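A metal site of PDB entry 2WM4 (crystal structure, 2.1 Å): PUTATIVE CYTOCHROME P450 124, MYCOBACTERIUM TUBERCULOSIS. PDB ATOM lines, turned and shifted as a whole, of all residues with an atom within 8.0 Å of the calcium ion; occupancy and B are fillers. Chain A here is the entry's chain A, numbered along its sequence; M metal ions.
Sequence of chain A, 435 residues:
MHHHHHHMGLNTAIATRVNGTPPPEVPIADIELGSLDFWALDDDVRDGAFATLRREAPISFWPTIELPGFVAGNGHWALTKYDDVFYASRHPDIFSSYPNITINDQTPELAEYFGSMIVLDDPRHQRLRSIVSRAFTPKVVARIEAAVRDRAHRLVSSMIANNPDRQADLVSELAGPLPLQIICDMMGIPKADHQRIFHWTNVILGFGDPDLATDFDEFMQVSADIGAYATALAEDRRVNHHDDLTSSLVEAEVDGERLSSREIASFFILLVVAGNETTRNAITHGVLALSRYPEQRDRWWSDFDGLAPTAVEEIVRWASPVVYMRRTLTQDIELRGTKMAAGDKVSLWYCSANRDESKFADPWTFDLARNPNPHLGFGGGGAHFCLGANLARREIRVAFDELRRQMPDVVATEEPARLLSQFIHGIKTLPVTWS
The side-chain carboxylate (OE2) of Glu 173 sits at hydrogen-bond distance from the side-chain amide nitrogen (ND2) of Asn 163 (2.9 Å).
The backbone carbonyl oxygen (O) of Met 159 is in hydrogen-bond range of the side-chain amide nitrogen (ND2) of Asn 163 (2.7 Å).
Within 4 Å of the calcium ion: Asn 163, Asp 165 and Gln 167.
The nearest printed residue that does not touch the calcium ion is Ala 168 (4.6 Å).
The calcium ion is bound by the backbone carbonyl oxygen (O) of Gln 167 (2.4 Å).
OD1 of Asn 163 binds the calcium ion (2.5 Å).
The side-chain carboxylate (OD2) of Asp 165 binds the calcium ion, at 2.6 Å.
The calcium ion is bound by OD1 of Asp 165 (2.7 Å).
The calcium ion has four donor atoms within binding distance.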
ATOM      1  N   MET A 159      -9.184  -6.112  -7.918  1.00  0.00           N
ATOM      2  CA  MET A 159     -10.381  -5.291  -8.062  1.00  0.00           C
ATOM      3  C   MET A 159     -10.522  -4.310  -6.924  1.00  0.00           C
ATOM      4  O   MET A 159     -10.826  -3.140  -7.165  1.00  0.00           O
ATOM      5  CB  MET A 159     -11.654  -6.140  -8.206  1.00  0.00           C
ATOM      6  CG  MET A 159     -12.894  -5.377  -8.616  1.00  0.00           C
ATOM      7  SD  MET A 159     -14.313  -6.513  -8.919  1.00  0.00           S
ATOM      8  CE  MET A 159     -15.648  -5.518  -8.383  1.00  0.00           C
ATOM      9  N   ILE A 160     -10.275  -4.791  -5.686  1.00  0.00           N
ATOM     10  CA  ILE A 160     -10.290  -3.928  -4.491  1.00  0.00           C
ATOM     11  C   ILE A 160      -9.096  -2.952  -4.545  1.00  0.00           C
ATOM     12  O   ILE A 160      -9.294  -1.729  -4.442  1.00  0.00           O
ATOM     13  CB  ILE A 160     -10.267  -4.759  -3.183  1.00  0.00           C
ATOM     14  CG1 ILE A 160     -11.561  -5.578  -3.011  1.00  0.00           C
ATOM     15  CG2 ILE A 160     -10.107  -3.886  -1.963  1.00  0.00           C
ATOM     16  CD1 ILE A 160     -11.492  -6.617  -1.911  1.00  0.00           C
ATOM     17  N   ASN A 162      -7.270  -1.869  -7.019  1.00  0.00           N
ATOM     18  CA  ASN A 162      -7.405  -0.964  -8.153  1.00  0.00           C
ATOM     19  C   ASN A 162      -8.415   0.131  -7.939  1.00  0.00           C
ATOM     20  O   ASN A 162      -8.359   1.121  -8.642  1.00  0.00           O
ATOM     21  CB  ASN A 162      -7.779  -1.716  -9.424  1.00  0.00           C
ATOM     22  CG  ASN A 162      -6.640  -2.542  -9.930  1.00  0.00           C
ATOM     23  OD1 ASN A 162      -5.535  -2.452  -9.417  1.00  0.00           O
ATOM     24  ND2 ASN A 162      -6.905  -3.359 -10.945  1.00  0.00           N
ATOM     25  N   ASN A 163      -9.299  -0.033  -6.959  1.00  0.00           N
ATOM     26  CA  ASN A 163     -10.481   0.818  -6.790  1.00  0.00           C
ATOM     27  C   ASN A 163     -10.706   1.387  -5.405  1.00  0.00           C
ATOM     28  O   ASN A 163     -11.594   0.941  -4.659  1.00  0.00           O
ATOM     29  CB  ASN A 163     -11.721   0.074  -7.315  1.00  0.00           C
ATOM     30  CG  ASN A 163     -11.644  -0.193  -8.753  1.00  0.00           C
ATOM     31  OD1 ASN A 163     -11.762   0.722  -9.564  1.00  0.00           O
ATOM     32  ND2 ASN A 163     -11.350  -1.416  -9.115  1.00  0.00           N
ATOM     33  N   PRO A 164      -9.915   2.415  -5.024  1.00  0.00           N
ATOM     34  CA  PRO A 164     -10.109   3.066  -3.736  1.00  0.00           C
ATOM     35  C   PRO A 164     -11.505   3.625  -3.594  1.00  0.00           C
ATOM     36  O   PRO A 164     -12.047   3.633  -2.479  1.00  0.00           O
ATOM     37  CB  PRO A 164      -9.111   4.230  -3.786  1.00  0.00           C
ATOM     38  CG  PRO A 164      -8.170   3.913  -4.885  1.00  0.00           C
ATOM     39  CD  PRO A 164      -8.914   3.101  -5.858  1.00  0.00           C
ATOM     40  N   ASP A 165     -12.094   4.106  -4.722  1.00  0.00           N
ATOM     41  CA  ASP A 165     -13.482   4.585  -4.759  1.00  0.00           C
ATOM     42  C   ASP A 165     -14.568   3.516  -4.502  1.00  0.00           C
ATOM     43  O   ASP A 165     -15.743   3.857  -4.386  1.00  0.00           O
ATOM     44  CB  ASP A 165     -13.807   5.238  -6.103  1.00  0.00           C
ATOM     45  CG  ASP A 165     -13.446   4.378  -7.309  1.00  0.00           C
ATOM     46  OD1 ASP A 165     -12.975   3.229  -7.202  1.00  0.00           O
ATOM     47  OD2 ASP A 165     -13.669   4.905  -8.409  1.00  0.00           O
ATOM     48  N   ARG A 166     -14.158   2.238  -4.458  1.00  0.00           N
ATOM     49  CA  ARG A 166     -15.121   1.127  -4.343  1.00  0.00           C
ATOM     50  C   ARG A 166     -16.141   1.123  -5.488  1.00  0.00           C
ATOM     51  O   ARG A 166     -17.304   0.793  -5.299  1.00  0.00           O
ATOM     52  CB  ARG A 166     -15.781   1.142  -2.951  1.00  0.00           C
ATOM     53  CG  ARG A 166     -14.696   0.740  -1.899  1.00  0.00           C
ATOM     54  CD  ARG A 166     -15.253   0.617  -0.484  1.00  0.00           C
ATOM     55  NE  ARG A 166     -15.912   1.869  -0.069  1.00  0.00           N
ATOM     56  CZ  ARG A 166     -16.462   2.067   1.129  1.00  0.00           C
ATOM     57  NH1 ARG A 166     -16.396   1.107   2.044  1.00  0.00           N
ATOM     58  NH2 ARG A 166     -17.055   3.218   1.394  1.00  0.00           N
ATOM     59  N   GLN A 167     -15.664   1.509  -6.665  1.00  0.00           N
ATOM     60  CA  GLN A 167     -16.467   1.602  -7.903  1.00  0.00           C
ATOM     61  C   GLN A 167     -15.663   0.939  -8.978  1.00  0.00           C
ATOM     62  O   GLN A 167     -14.590   1.375  -9.307  1.00  0.00           O
ATOM     63  CB  GLN A 167     -16.703   3.065  -8.309  1.00  0.00           C
ATOM     64  CG  GLN A 167     -17.719   3.835  -7.389  1.00  0.00           C
ATOM     65  CD  GLN A 167     -17.913   5.301  -7.843  1.00  0.00           C
ATOM     66  OE1 GLN A 167     -17.082   6.182  -7.543  1.00  0.00           O
ATOM     67  NE2 GLN A 167     -18.972   5.548  -8.616  1.00  0.00           N
ATOM     68  N   ALA A 168     -16.128  -0.193  -9.490  1.00  0.00           N
ATOM     69  CA  ALA A 168     -15.369  -0.820 -10.539  1.00  0.00           C
ATOM     70  C   ALA A 168     -16.274  -1.296 -11.643  1.00  0.00           C
ATOM     71  O   ALA A 168     -17.483  -1.443 -11.429  1.00  0.00           O
ATOM     72  CB  ALA A 168     -14.552  -2.013  -9.968  1.00  0.00           C
ATOM     73  N   ASP A 169     -15.678  -1.615 -12.796  1.00  0.00           N
ATOM     74  CA  ASP A 169     -16.381  -2.355 -13.849  1.00  0.00           C
ATOM     75  C   ASP A 169     -16.145  -3.830 -13.600  1.00  0.00           C
ATOM     76  O   ASP A 169     -15.010  -4.321 -13.744  1.00  0.00           O
ATOM     77  CB  ASP A 169     -15.853  -1.983 -15.249  1.00  0.00           C
ATOM     78  CG  ASP A 169     -16.338  -2.950 -16.328  1.00  0.00           C
ATOM     79  OD1 ASP A 169     -15.594  -3.226 -17.277  1.00  0.00           O
ATOM     80  OD2 ASP A 169     -17.455  -3.457 -16.279  1.00  0.00           O
ATOM     81  N   GLU A 173     -12.728  -6.166 -14.567  1.00  0.00           N
ATOM     82  CA  GLU A 173     -11.882  -6.402 -13.374  1.00  0.00           C
ATOM     83  C   GLU A 173     -11.889  -7.862 -12.951  1.00  0.00           C
ATOM     84  O   GLU A 173     -10.916  -8.310 -12.353  1.00  0.00           O
ATOM     85  CB  GLU A 173     -12.254  -5.529 -12.171  1.00  0.00           C
ATOM     86  CG  GLU A 173     -12.196  -4.062 -12.455  1.00  0.00           C
ATOM     87  CD  GLU A 173     -10.910  -3.385 -11.959  1.00  0.00           C
ATOM     88  OE1 GLU A 173      -9.878  -4.055 -11.644  1.00  0.00           O
ATOM     89  OE2 GLU A 173     -10.961  -2.156 -11.911  1.00  0.00           O
ATOM     90  N   VAL A 432     -20.052  -1.757 -10.687  1.00  0.00           N
ATOM     91  CA  VAL A 432     -20.458  -2.313  -9.399  1.00  0.00           C
ATOM     92  C   VAL A 432     -19.832  -1.489  -8.264  1.00  0.00           C
ATOM     93  O   VAL A 432     -18.894  -0.740  -8.474  1.00  0.00           O
ATOM     94  CB  VAL A 432     -20.078  -3.805  -9.229  1.00  0.00           C
ATOM     95  CG1 VAL A 432     -20.815  -4.713 -10.279  1.00  0.00           C
ATOM     96  CG2 VAL A 432     -18.582  -3.999  -9.337  1.00  0.00           C
ATOM     97  N   TRP A 434     -19.271  -1.826  -3.693  1.00  0.00           N
ATOM     98  CA  TRP A 434     -19.279  -2.685  -2.491  1.00  0.00           C
ATOM     99  C   TRP A 434     -18.887  -1.819  -1.266  1.00  0.00           C
ATOM    100  O   TRP A 434     -18.469  -0.690  -1.440  1.00  0.00           O
ATOM    101  CB  TRP A 434     -18.275  -3.875  -2.654  1.00  0.00           C
ATOM    102  CG  TRP A 434     -16.826  -3.437  -2.811  1.00  0.00           C
ATOM    103  CD1 TRP A 434     -15.915  -3.229  -1.821  1.00  0.00           C
ATOM    104  CD2 TRP A 434     -16.167  -3.056  -4.059  1.00  0.00           C
ATOM    105  NE1 TRP A 434     -14.729  -2.791  -2.371  1.00  0.00           N
ATOM    106  CE2 TRP A 434     -14.866  -2.669  -3.737  1.00  0.00           C
ATOM    107  CE3 TRP A 434     -16.583  -3.015  -5.396  1.00  0.00           C
ATOM    108  CZ2 TRP A 434     -13.935  -2.278  -4.715  1.00  0.00           C
ATOM    109  CZ3 TRP A 434     -15.654  -2.601  -6.371  1.00  0.00           C
ATOM    110  CH2 TRP A 434     -14.346  -2.232  -6.017  1.00  0.00           C
HETATM  111 CA    CA M   1     -12.825   2.937  -9.852  1.00  0.00          CA
